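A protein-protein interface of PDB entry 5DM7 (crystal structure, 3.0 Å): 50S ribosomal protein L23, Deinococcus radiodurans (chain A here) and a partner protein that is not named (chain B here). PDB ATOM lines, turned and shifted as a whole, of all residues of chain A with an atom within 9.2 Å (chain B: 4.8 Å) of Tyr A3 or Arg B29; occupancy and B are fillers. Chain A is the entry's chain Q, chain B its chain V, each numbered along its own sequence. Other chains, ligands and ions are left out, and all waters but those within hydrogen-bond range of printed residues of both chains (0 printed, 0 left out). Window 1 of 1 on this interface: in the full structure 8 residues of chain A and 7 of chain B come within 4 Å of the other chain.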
ATOM      1  N   SER A   1     -16.685 -18.508  -3.796  1.00  0.00           N
ATOM      2  CA  SER A   1     -16.923 -18.714  -2.377  1.00  0.00           C
ATOM      3  C   SER A   1     -18.090 -19.657  -2.159  1.00  0.00           C
ATOM      4  O   SER A   1     -18.380 -20.518  -2.991  1.00  0.00           O
ATOM      5  CB  SER A   1     -17.229 -17.387  -1.678  1.00  0.00           C
ATOM      6  OG  SER A   1     -18.631 -17.187  -1.559  1.00  0.00           O
ATOM      7  N   HIS A   2     -18.787 -19.442  -1.048  1.00  0.00           N
ATOM      8  CA  HIS A   2     -19.882 -20.293  -0.581  1.00  0.00           C
ATOM      9  C   HIS A   2     -21.035 -20.438  -1.574  1.00  0.00           C
ATOM     10  O   HIS A   2     -22.185 -20.616  -1.173  1.00  0.00           O
ATOM     11  CB  HIS A   2     -20.421 -19.729   0.738  1.00  0.00           C
ATOM     12  CG  HIS A   2     -19.462 -18.811   1.434  1.00  0.00           C
ATOM     13  ND1 HIS A   2     -18.413 -19.271   2.203  1.00  0.00           N
ATOM     14  CD2 HIS A   2     -19.386 -17.459   1.468  1.00  0.00           C
ATOM     15  CE1 HIS A   2     -17.740 -18.243   2.688  1.00  0.00           C
ATOM     16  NE2 HIS A   2     -18.309 -17.132   2.256  1.00  0.00           N
ATOM     17  N   TYR A   3     -20.712 -20.362  -2.861  1.00  0.00           N
ATOM     18  CA  TYR A   3     -21.685 -20.448  -3.939  1.00  0.00           C
ATOM     19  C   TYR A   3     -20.983 -20.973  -5.177  1.00  0.00           C
ATOM     20  O   TYR A   3     -21.362 -22.014  -5.714  1.00  0.00           O
ATOM     21  CB  TYR A   3     -22.278 -19.070  -4.267  1.00  0.00           C
ATOM     22  CG  TYR A   3     -23.248 -18.513  -3.242  1.00  0.00           C
ATOM     23  CD1 TYR A   3     -24.434 -19.183  -2.935  1.00  0.00           C
ATOM     24  CD2 TYR A   3     -22.995 -17.303  -2.603  1.00  0.00           C
ATOM     25  CE1 TYR A   3     -25.328 -18.671  -2.005  1.00  0.00           C
ATOM     26  CE2 TYR A   3     -23.885 -16.781  -1.674  1.00  0.00           C
ATOM     27  CZ  TYR A   3     -25.048 -17.469  -1.379  1.00  0.00           C
ATOM     28  OH  TYR A   3     -25.928 -16.950  -0.457  1.00  0.00           O
ATOM     29  N   ASP A   4     -19.969 -20.221  -5.611  1.00  0.00           N
ATOM     30  CA  ASP A   4     -19.150 -20.505  -6.788  1.00  0.00           C
ATOM     31  C   ASP A   4     -19.059 -21.995  -7.063  1.00  0.00           C
ATOM     32  O   ASP A   4     -19.333 -22.467  -8.167  1.00  0.00           O
ATOM     33  CB  ASP A   4     -17.735 -19.956  -6.551  1.00  0.00           C
ATOM     34  CG  ASP A   4     -17.250 -19.026  -7.670  1.00  0.00           C
ATOM     35  OD1 ASP A   4     -17.775 -19.112  -8.804  1.00  0.00           O
ATOM     36  OD2 ASP A   4     -16.326 -18.215  -7.414  1.00  0.00           O
ATOM     37  N   ILE A   5     -18.706 -22.715  -6.003  1.00  0.00           N
ATOM     38  CA  ILE A   5     -18.479 -24.161  -5.991  1.00  0.00           C
ATOM     39  C   ILE A   5     -19.569 -25.016  -6.667  1.00  0.00           C
ATOM     40  O   ILE A   5     -19.254 -25.875  -7.490  1.00  0.00           O
ATOM     41  CB  ILE A   5     -18.213 -24.636  -4.521  1.00  0.00           C
ATOM     42  CG1 ILE A   5     -16.710 -24.768  -4.249  1.00  0.00           C
ATOM     43  CG2 ILE A   5     -18.921 -25.934  -4.201  1.00  0.00           C
ATOM     44  CD1 ILE A   5     -16.375 -24.854  -2.775  1.00  0.00           C
ATOM     45  N   LEU A   6     -20.836 -24.766  -6.346  1.00  0.00           N
ATOM     46  CA  LEU A   6     -21.923 -25.655  -6.761  1.00  0.00           C
ATOM     47  C   LEU A   6     -22.344 -25.440  -8.206  1.00  0.00           C
ATOM     48  O   LEU A   6     -23.469 -25.052  -8.480  1.00  0.00           O
ATOM     49  CB  LEU A   6     -23.124 -25.516  -5.823  1.00  0.00           C
ATOM     50  CG  LEU A   6     -22.835 -25.885  -4.362  1.00  0.00           C
ATOM     51  CD1 LEU A   6     -22.372 -24.676  -3.555  1.00  0.00           C
ATOM     52  CD2 LEU A   6     -24.036 -26.551  -3.701  1.00  0.00           C
ATOM     53  N   GLN A   7     -21.434 -25.745  -9.122  1.00  0.00           N
ATOM     54  CA  GLN A   7     -21.569 -25.413 -10.541  1.00  0.00           C
ATOM     55  C   GLN A   7     -22.881 -25.765 -11.249  1.00  0.00           C
ATOM     56  O   GLN A   7     -23.040 -25.372 -12.404  1.00  0.00           O
ATOM     57  CB  GLN A   7     -20.393 -25.992 -11.350  1.00  0.00           C
ATOM     58  CG  GLN A   7     -19.130 -25.119 -11.387  1.00  0.00           C
ATOM     59  CD  GLN A   7     -17.968 -25.766 -12.159  1.00  0.00           C
ATOM     60  OE1 GLN A   7     -17.321 -25.111 -12.985  1.00  0.00           O
ATOM     61  NE2 GLN A   7     -17.695 -27.048 -11.882  1.00  0.00           N
ATOM     62  N   ALA A   8     -23.791 -26.487 -10.580  1.00  0.00           N
ATOM     63  CA  ALA A   8     -25.101 -26.894 -11.146  1.00  0.00           C
ATOM     64  C   ALA A   8     -25.839 -27.956 -10.316  1.00  0.00           C
ATOM     65  O   ALA A   8     -25.298 -28.478  -9.346  1.00  0.00           O
ATOM     66  CB  ALA A   8     -24.948 -27.409 -12.587  1.00  0.00           C
ATOM     67  N   PRO A   9     -27.085 -28.284 -10.702  1.00  0.00           N
ATOM     68  CA  PRO A   9     -27.722 -29.462 -10.110  1.00  0.00           C
ATOM     69  C   PRO A   9     -27.751 -30.611 -11.107  1.00  0.00           C
ATOM     70  O   PRO A   9     -27.484 -30.406 -12.289  1.00  0.00           O
ATOM     71  CB  PRO A   9     -29.144 -28.977  -9.870  1.00  0.00           C
ATOM     72  CG  PRO A   9     -29.399 -28.115 -11.061  1.00  0.00           C
ATOM     73  CD  PRO A   9     -28.077 -27.425 -11.373  1.00  0.00           C
ATOM     74  N   ILE A  11     -29.585 -33.802 -13.160  1.00  0.00           N
ATOM     75  CA  ILE A  11     -30.905 -33.992 -13.758  1.00  0.00           C
ATOM     76  C   ILE A  11     -31.115 -35.369 -14.408  1.00  0.00           C
ATOM     77  O   ILE A  11     -30.527 -35.649 -15.449  1.00  0.00           O
ATOM     78  CB  ILE A  11     -31.164 -32.907 -14.833  1.00  0.00           C
ATOM     79  CG1 ILE A  11     -30.839 -31.515 -14.291  1.00  0.00           C
ATOM     80  CG2 ILE A  11     -32.599 -32.971 -15.331  1.00  0.00           C
ATOM     81  CD1 ILE A  11     -29.423 -31.071 -14.553  1.00  0.00           C
ATOM     82  N   TRP A  27     -23.781 -31.330  -9.712  1.00  0.00           N
ATOM     83  CA  TRP A  27     -22.414 -31.255 -10.221  1.00  0.00           C
ATOM     84  C   TRP A  27     -21.690 -30.232  -9.358  1.00  0.00           C
ATOM     85  O   TRP A  27     -22.307 -29.326  -8.826  1.00  0.00           O
ATOM     86  CB  TRP A  27     -22.362 -30.812 -11.681  1.00  0.00           C
ATOM     87  CG  TRP A  27     -23.001 -31.752 -12.645  1.00  0.00           C
ATOM     88  CD1 TRP A  27     -24.053 -31.486 -13.469  1.00  0.00           C
ATOM     89  CD2 TRP A  27     -22.626 -33.111 -12.898  1.00  0.00           C
ATOM     90  NE1 TRP A  27     -24.364 -32.593 -14.218  1.00  0.00           N
ATOM     91  CE2 TRP A  27     -23.500 -33.605 -13.890  1.00  0.00           C
ATOM     92  CE3 TRP A  27     -21.640 -33.961 -12.383  1.00  0.00           C
ATOM     93  CZ2 TRP A  27     -23.414 -34.915 -14.380  1.00  0.00           C
ATOM     94  CZ3 TRP A  27     -21.561 -35.257 -12.866  1.00  0.00           C
ATOM     95  CH2 TRP A  27     -22.447 -35.723 -13.851  1.00  0.00           C
ATOM     96  N   VAL A  28     -20.387 -30.380  -9.194  1.00  0.00           N
ATOM     97  CA  VAL A  28     -19.626 -29.483  -8.328  1.00  0.00           C
ATOM     98  C   VAL A  28     -18.332 -29.061  -9.068  1.00  0.00           C
ATOM     99  O   VAL A  28     -18.338 -28.923 -10.301  1.00  0.00           O
ATOM    100  CB  VAL A  28     -19.390 -30.132  -6.909  1.00  0.00           C
ATOM    101  CG1 VAL A  28     -18.912 -29.132  -5.882  1.00  0.00           C
ATOM    102  CG2 VAL A  28     -20.666 -30.722  -6.388  1.00  0.00           C
ATOM    103  N   SER A  29     -17.237 -28.861  -8.335  1.00  0.00           N
ATOM    104  CA  SER A  29     -16.013 -28.290  -8.888  1.00  0.00           C
ATOM    105  C   SER A  29     -14.836 -29.199  -8.603  1.00  0.00           C
ATOM    106  O   SER A  29     -14.357 -29.235  -7.472  1.00  0.00           O
ATOM    107  CB  SER A  29     -15.745 -26.919  -8.260  1.00  0.00           C
ATOM    108  OG  SER A  29     -16.230 -25.868  -9.075  1.00  0.00           O
ATOM    109  N   GLU A  36     -15.273 -29.135   2.061  1.00  0.00           N
ATOM    110  CA  GLU A  36     -15.630 -27.919   1.320  1.00  0.00           C
ATOM    111  C   GLU A  36     -17.082 -27.944   0.823  1.00  0.00           C
ATOM    112  O   GLU A  36     -17.793 -26.950   0.941  1.00  0.00           O
ATOM    113  CB  GLU A  36     -14.671 -27.676   0.142  1.00  0.00           C
ATOM    114  CG  GLU A  36     -13.289 -27.117   0.518  1.00  0.00           C
ATOM    115  CD  GLU A  36     -12.256 -27.203  -0.629  1.00  0.00           C
ATOM    116  OE1 GLU A  36     -12.596 -27.695  -1.731  1.00  0.00           O
ATOM    117  OE2 GLU A  36     -11.094 -26.781  -0.426  1.00  0.00           O
ATOM    118  N   ILE A  37     -17.522 -29.073   0.273  1.00  0.00           N
ATOM    119  CA  ILE A  37     -18.889 -29.173  -0.223  1.00  0.00           C
ATOM    120  C   ILE A  37     -19.880 -29.139   0.932  1.00  0.00           C
ATOM    121  O   ILE A  37     -20.936 -28.502   0.833  1.00  0.00           O
ATOM    122  CB  ILE A  37     -19.107 -30.435  -1.070  1.00  0.00           C
ATOM    123  CG1 ILE A  37     -18.265 -30.369  -2.343  1.00  0.00           C
ATOM    124  CG2 ILE A  37     -20.561 -30.558  -1.457  1.00  0.00           C
ATOM    125  CD1 ILE A  37     -18.291 -31.634  -3.156  1.00  0.00           C
ATOM    126  N   ASP A  39     -19.471 -27.683   3.947  1.00  0.00           N
ATOM    127  CA  ASP A  39     -19.517 -26.275   4.309  1.00  0.00           C
ATOM    128  C   ASP A  39     -20.363 -25.475   3.305  1.00  0.00           C
ATOM    129  O   ASP A  39     -21.153 -24.615   3.706  1.00  0.00           O
ATOM    130  CB  ASP A  39     -18.096 -25.712   4.445  1.00  0.00           C
ATOM    131  CG  ASP A  39     -17.885 -24.420   3.658  1.00  0.00           C
ATOM    132  OD1 ASP A  39     -17.088 -24.439   2.689  1.00  0.00           O
ATOM    133  OD2 ASP A  39     -18.503 -23.387   4.014  1.00  0.00           O
ATOM    134  N   ALA A  40     -20.224 -25.793   2.018  1.00  0.00           N
ATOM    135  CA  ALA A  40     -20.946 -25.095   0.957  1.00  0.00           C
ATOM    136  C   ALA A  40     -22.451 -25.190   1.129  1.00  0.00           C
ATOM    137  O   ALA A  40     -23.133 -24.181   1.371  1.00  0.00           O
ATOM    138  CB  ALA A  40     -20.551 -25.630  -0.404  1.00  0.00           C
ATOM    139  N   ILE A  41     -22.980 -26.402   1.015  1.00  0.00           N
ATOM    140  CA  ILE A  41     -24.431 -26.556   1.037  1.00  0.00           C
ATOM    141  C   ILE A  41     -25.032 -26.252   2.406  1.00  0.00           C
ATOM    142  O   ILE A  41     -26.121 -25.690   2.492  1.00  0.00           O
ATOM    143  CB  ILE A  41     -24.858 -27.936   0.555  1.00  0.00           C
ATOM    144  CG1 ILE A  41     -23.801 -28.487  -0.399  1.00  0.00           C
ATOM    145  CG2 ILE A  41     -26.226 -27.850  -0.117  1.00  0.00           C
ATOM    146  CD1 ILE A  41     -24.153 -29.815  -1.004  1.00  0.00           C
ATOM    147  N   GLN A  43     -23.989 -23.985   4.299  1.00  0.00           N
ATOM    148  CA  GLN A  43     -24.073 -22.522   4.316  1.00  0.00           C
ATOM    149  C   GLN A  43     -25.229 -21.958   3.493  1.00  0.00           C
ATOM    150  O   GLN A  43     -26.056 -21.200   4.006  1.00  0.00           O
ATOM    151  CB  GLN A  43     -22.767 -21.889   3.832  1.00  0.00           C
ATOM    152  CG  GLN A  43     -21.737 -21.660   4.922  1.00  0.00           C
ATOM    153  CD  GLN A  43     -20.831 -20.477   4.621  1.00  0.00           C
ATOM    154  OE1 GLN A  43     -21.236 -19.527   3.942  1.00  0.00           O
ATOM    155  NE2 GLN A  43     -19.597 -20.531   5.124  1.00  0.00           N
ATOM    156  N   ALA A  44     -25.275 -22.310   2.212  1.00  0.00           N
ATOM    157  CA  ALA A  44     -26.246 -21.690   1.322  1.00  0.00           C
ATOM    158  C   ALA A  44     -27.571 -22.436   1.264  1.00  0.00           C
ATOM    159  O   ALA A  44     -28.371 -22.196   0.370  1.00  0.00           O
ATOM    160  CB  ALA A  44     -25.671 -21.525  -0.066  1.00  0.00           C
ATOM    161  N   PHE A  45     -27.815 -23.335   2.210  1.00  0.00           N
ATOM    162  CA  PHE A  45     -29.118 -23.997   2.276  1.00  0.00           C
ATOM    163  C   PHE A  45     -29.634 -24.236   3.680  1.00  0.00           C
ATOM    164  O   PHE A  45     -30.667 -24.880   3.848  1.00  0.00           O
ATOM    165  CB  PHE A  45     -29.106 -25.319   1.519  1.00  0.00           C
ATOM    166  CG  PHE A  45     -29.246 -25.158   0.053  1.00  0.00           C
ATOM    167  CD1 PHE A  45     -28.137 -24.918  -0.734  1.00  0.00           C
ATOM    168  CD2 PHE A  45     -30.488 -25.238  -0.540  1.00  0.00           C
ATOM    169  CE1 PHE A  45     -28.263 -24.757  -2.083  1.00  0.00           C
ATOM    170  CE2 PHE A  45     -30.626 -25.078  -1.890  1.00  0.00           C
ATOM    171  CZ  PHE A  45     -29.512 -24.839  -2.667  1.00  0.00           C
ATOM    172  N   GLY A  46     -28.911 -23.722   4.672  1.00  0.00           N
ATOM    173  CA  GLY A  46     -29.298 -23.842   6.068  1.00  0.00           C
ATOM    174  C   GLY A  46     -29.794 -25.221   6.484  1.00  0.00           C
ATOM    175  O   GLY A  46     -30.872 -25.356   7.073  1.00  0.00           O
ATOM    176  N   ASP B  19     -20.588 -11.300  -2.666  1.00  0.00           N
ATOM    177  CA  ASP B  19     -21.331 -12.481  -2.224  1.00  0.00           C
ATOM    178  C   ASP B  19     -22.726 -12.602  -2.859  1.00  0.00           C
ATOM    179  O   ASP B  19     -23.078 -13.642  -3.418  1.00  0.00           O
ATOM    180  CB  ASP B  19     -21.429 -12.529  -0.690  1.00  0.00           C
ATOM    181  CG  ASP B  19     -21.905 -13.890  -0.161  1.00  0.00           C
ATOM    182  OD1 ASP B  19     -23.137 -14.110  -0.079  1.00  0.00           O
ATOM    183  OD2 ASP B  19     -21.045 -14.736   0.183  1.00  0.00           O
ATOM    184  N   LYS B  22     -22.678 -13.095  -6.676  1.00  0.00           N
ATOM    185  CA  LYS B  22     -22.410 -14.512  -6.840  1.00  0.00           C
ATOM    186  C   LYS B  22     -23.717 -15.258  -6.733  1.00  0.00           C
ATOM    187  O   LYS B  22     -24.160 -15.824  -7.707  1.00  0.00           O
ATOM    188  CB  LYS B  22     -21.459 -15.017  -5.756  1.00  0.00           C
ATOM    189  CG  LYS B  22     -20.007 -14.586  -5.892  1.00  0.00           C
ATOM    190  CD  LYS B  22     -19.232 -15.526  -6.796  1.00  0.00           C
ATOM    191  CE  LYS B  22     -17.730 -15.323  -6.656  1.00  0.00           C
ATOM    192  NZ  LYS B  22     -17.220 -14.084  -7.308  1.00  0.00           N
ATOM    193  N   LYS B  23     -24.339 -15.221  -5.553  1.00  0.00           N
ATOM    194  CA  LYS B  23     -25.565 -15.987  -5.264  1.00  0.00           C
ATOM    195  C   LYS B  23     -26.595 -15.951  -6.386  1.00  0.00           C
ATOM    196  O   LYS B  23     -27.128 -16.989  -6.805  1.00  0.00           O
ATOM    197  CB  LYS B  23     -26.216 -15.501  -3.964  1.00  0.00           C
ATOM    198  CG  LYS B  23     -27.580 -16.128  -3.670  1.00  0.00           C
ATOM    199  CD  LYS B  23     -28.231 -15.509  -2.427  1.00  0.00           C
ATOM    200  CE  LYS B  23     -29.654 -16.025  -2.196  1.00  0.00           C
ATOM    201  NZ  LYS B  23     -30.396 -15.195  -1.202  1.00  0.00           N
ATOM    202  N   LEU B  25     -25.922 -15.084  -9.451  1.00  0.00           N
ATOM    203  CA  LEU B  25     -25.276 -15.690 -10.599  1.00  0.00           C
ATOM    204  C   LEU B  25     -25.477 -17.212 -10.560  1.00  0.00           C
ATOM    205  O   LEU B  25     -25.746 -17.852 -11.586  1.00  0.00           O
ATOM    206  CB  LEU B  25     -23.794 -15.323 -10.612  1.00  0.00           C
ATOM    207  CG  LEU B  25     -23.028 -15.597 -11.900  1.00  0.00           C
ATOM    208  CD1 LEU B  25     -22.262 -16.922 -11.835  1.00  0.00           C
ATOM    209  CD2 LEU B  25     -23.985 -15.566 -13.089  1.00  0.00           C
ATOM    210  N   MET B  26     -25.380 -17.776  -9.359  1.00  0.00           N
ATOM    211  CA  MET B  26     -25.490 -19.214  -9.146  1.00  0.00           C
ATOM    212  C   MET B  26     -26.904 -19.702  -9.421  1.00  0.00           C
ATOM    213  O   MET B  26     -27.097 -20.671 -10.170  1.00  0.00           O
ATOM    214  CB  MET B  26     -25.078 -19.575  -7.717  1.00  0.00           C
ATOM    215  CG  MET B  26     -25.553 -20.945  -7.282  1.00  0.00           C
ATOM    216  SD  MET B  26     -26.002 -20.999  -5.535  1.00  0.00           S
ATOM    217  CE  MET B  26     -27.223 -22.312  -5.522  1.00  0.00           C
ATOM    218  N   GLU B  27     -27.888 -19.032  -8.819  1.00  0.00           N
ATOM    219  CA  GLU B  27     -29.290 -19.412  -9.016  1.00  0.00           C
ATOM    220  C   GLU B  27     -29.631 -19.333 -10.497  1.00  0.00           C
ATOM    221  O   GLU B  27     -30.389 -20.151 -11.032  1.00  0.00           O
ATOM    222  CB  GLU B  27     -30.226 -18.491  -8.236  1.00  0.00           C
ATOM    223  CG  GLU B  27     -30.092 -18.532  -6.721  1.00  0.00           C
ATOM    224  CD  GLU B  27     -30.895 -17.417  -6.054  1.00  0.00           C
ATOM    225  OE1 GLU B  27     -31.187 -17.523  -4.840  1.00  0.00           O
ATOM    226  OE2 GLU B  27     -31.235 -16.431  -6.752  1.00  0.00           O
ATOM    227  N   LEU B  28     -29.060 -18.323 -11.144  1.00  0.00           N
ATOM    228  CA  LEU B  28     -29.158 -18.159 -12.582  1.00  0.00           C
ATOM    229  C   LEU B  28     -28.663 -19.407 -13.284  1.00  0.00           C
ATOM    230  O   LEU B  28     -29.311 -19.894 -14.203  1.00  0.00           O
ATOM    231  CB  LEU B  28     -28.312 -16.974 -13.037  1.00  0.00           C
ATOM    232  CG  LEU B  28     -28.921 -15.581 -13.060  1.00  0.00           C
ATOM    233  CD1 LEU B  28     -27.817 -14.561 -12.906  1.00  0.00           C
ATOM    234  CD2 LEU B  28     -29.658 -15.371 -14.371  1.00  0.00           C
ATOM    235  N   ARG B  29     -27.501 -19.907 -12.859  1.00  0.00           N
ATOM    236  CA  ARG B  29     -26.932 -21.113 -13.461  1.00  0.00           C
ATOM    237  C   ARG B  29     -27.890 -22.283 -13.330  1.00  0.00           C
ATOM    238  O   ARG B  29     -28.251 -22.928 -14.320  1.00  0.00           O
ATOM    239  CB  ARG B  29     -25.598 -21.477 -12.807  1.00  0.00           C
ATOM    240  CG  ARG B  29     -24.491 -20.462 -13.025  1.00  0.00           C
ATOM    241  CD  ARG B  29     -23.170 -20.996 -12.512  1.00  0.00           C
ATOM    242  NE  ARG B  29     -23.248 -21.414 -11.113  1.00  0.00           N
ATOM    243  CZ  ARG B  29     -22.563 -20.847 -10.123  1.00  0.00           C
ATOM    244  NH1 ARG B  29     -21.744 -19.832 -10.376  1.00  0.00           N
ATOM    245  NH2 ARG B  29     -22.688 -21.295  -8.880  1.00  0.00           N
ATOM    246  N   PHE B  30     -28.295 -22.542 -12.093  1.00  0.00           N
ATOM    247  CA  PHE B  30     -29.222 -23.622 -11.801  1.00  0.00           C
ATOM    248  C   PHE B  30     -30.433 -23.550 -12.711  1.00  0.00           C
ATOM    249  O   PHE B  30     -30.831 -24.553 -13.306  1.00  0.00           O
ATOM    250  CB  PHE B  30     -29.648 -23.568 -10.337  1.00  0.00           C
ATOM    251  CG  PHE B  30     -28.629 -24.136  -9.396  1.00  0.00           C
ATOM    252  CD1 PHE B  30     -28.939 -25.219  -8.587  1.00  0.00           C
ATOM    253  CD2 PHE B  30     -27.351 -23.605  -9.336  1.00  0.00           C
ATOM    254  CE1 PHE B  30     -27.994 -25.753  -7.723  1.00  0.00           C
ATOM    255  CE2 PHE B  30     -26.405 -24.131  -8.481  1.00  0.00           C
ATOM    256  CZ  PHE B  30     -26.724 -25.208  -7.674  1.00  0.00           C
ATOM    257  N   GLN B  31     -31.001 -22.351 -12.826  1.00  0.00           N
ATOM    258  CA  GLN B  31     -32.057 -22.095 -13.794  1.00  0.00           C
ATOM    259  C   GLN B  31     -31.626 -22.562 -15.189  1.00  0.00           C
ATOM    260  O   GLN B  31     -32.283 -23.401 -15.805  1.00  0.00           O
ATOM    261  CB  GLN B  31     -32.402 -20.603 -13.839  1.00  0.00           C
ATOM    262  CG  GLN B  31     -33.231 -20.097 -12.670  1.00  0.00           C
ATOM    263  CD  GLN B  31     -34.078 -18.885 -13.051  1.00  0.00           C
ATOM    264  OE1 GLN B  31     -34.096 -18.474 -14.212  1.00  0.00           O
ATOM    265  NE2 GLN B  31     -34.790 -18.317 -12.076  1.00  0.00           N
ATOM    266  N   ALA B  32     -30.503 -22.029 -15.656  1.00  0.00           N
ATOM    267  CA  ALA B  32     -30.032 -22.241 -17.018  1.00  0.00           C
ATOM    268  C   ALA B  32     -30.002 -23.708 -17.390  1.00  0.00           C
ATOM    269  O   ALA B  32     -30.582 -24.110 -18.403  1.00  0.00           O
ATOM    270  CB  ALA B  32     -28.661 -21.622 -17.196  1.00  0.00           C
ATOM    271  N   ALA B  33     -29.342 -24.503 -16.551  1.00  0.00           N
ATOM    272  CA  ALA B  33     -29.228 -25.945 -16.786  1.00  0.00           C
ATOM    273  C   ALA B  33     -30.468 -26.714 -16.314  1.00  0.00           C
ATOM    274  O   ALA B  33     -30.526 -27.943 -16.425  1.00  0.00           O
ATOM    275  CB  ALA B  33     -27.958 -26.503 -16.147  1.00  0.00           C
ATOM    276  N   ALA B  34     -31.447 -25.986 -15.779  1.00  0.00           N
ATOM    277  CA  ALA B  34     -32.777 -26.545 -15.570  1.00  0.00           C
ATOM    278  C   ALA B  34     -33.668 -26.099 -16.720  1.00  0.00           C
ATOM    279  O   ALA B  34     -34.655 -26.756 -17.045  1.00  0.00           O
ATOM    280  CB  ALA B  34     -33.356 -26.092 -14.240  1.00  0.00           C
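The side-chain amide oxygen (OE1) of Gln A43 sits close to a ring nitrogen (ND1) of His A2, 3.3 Å away. The backbone carbonyl oxygen (O) of Ala A8 is in hydrogen-bond range of the backbone NH (N) of Trp A27, 3.3 Å away.
Among the printed residues, pairs that only touch across the chains: Ser A1 with Asp B19 (3.9 Å), His A2 with Asp B19 (3.4 Å), Tyr A3 with Asp B19 (3.2 Å), Tyr A3 with Lys B23 (3.4 Å), Tyr A3 with Met B26 (3.5 Å), Tyr A3 with Arg B29 (3.5 Å), Asp A4 with Lys B22 (3.3 Å), Asp A4 with Arg B29 (3.6 Å), Leu A6 with Arg B29 (3.9 Å), Leu A6 with Phe B30 (3.1 Å), Ala A8 with Phe B30 (3.9 Å), Pro A9 with Phe B30 (3.7 Å) and Ile A11 with Ala B33 (3.8 Å).
Printed residues of chain B within 4 Å of Asp A4: Lys B22 and Arg B29. Of the printed residues of chain B, Ala A8 touches Phe B30. Of the printed residues of chain A, Lys B22 touches Asp A4 (3.3 Å). Leu B25 touches none of the printed residues of chain A. Glu B27 touches none of the printed residues of chain A. Of chain A, only Tyr A3, Asp A4 and Leu A6 come within 4 Å of Arg B29. Printed residues of chain A within 4 Å of Phe B30: Leu A6, Ala A8 and Pro A9. No residue of chain A comes within 4 Å of Ala B32. Printed residues of chain A within 4 Å of Ala B33: Ile A11.
Hydrophobic or aromatic side chains of chain A within 4 Å of the printed part of chain B: His A2, Tyr A3, Pro A9 and Ile A11. Along chain A the printed residues that touch a printed residue of chain B span positions 1 to 11. Hydrophobic or aromatic side chains of chain B that line the printed part of chain A: Met B26 and Phe B30. Among the printed residues, no Asp or Glu carboxylate lies within 4 Å of a Lys or Arg side-chain nitrogen of the other chain.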
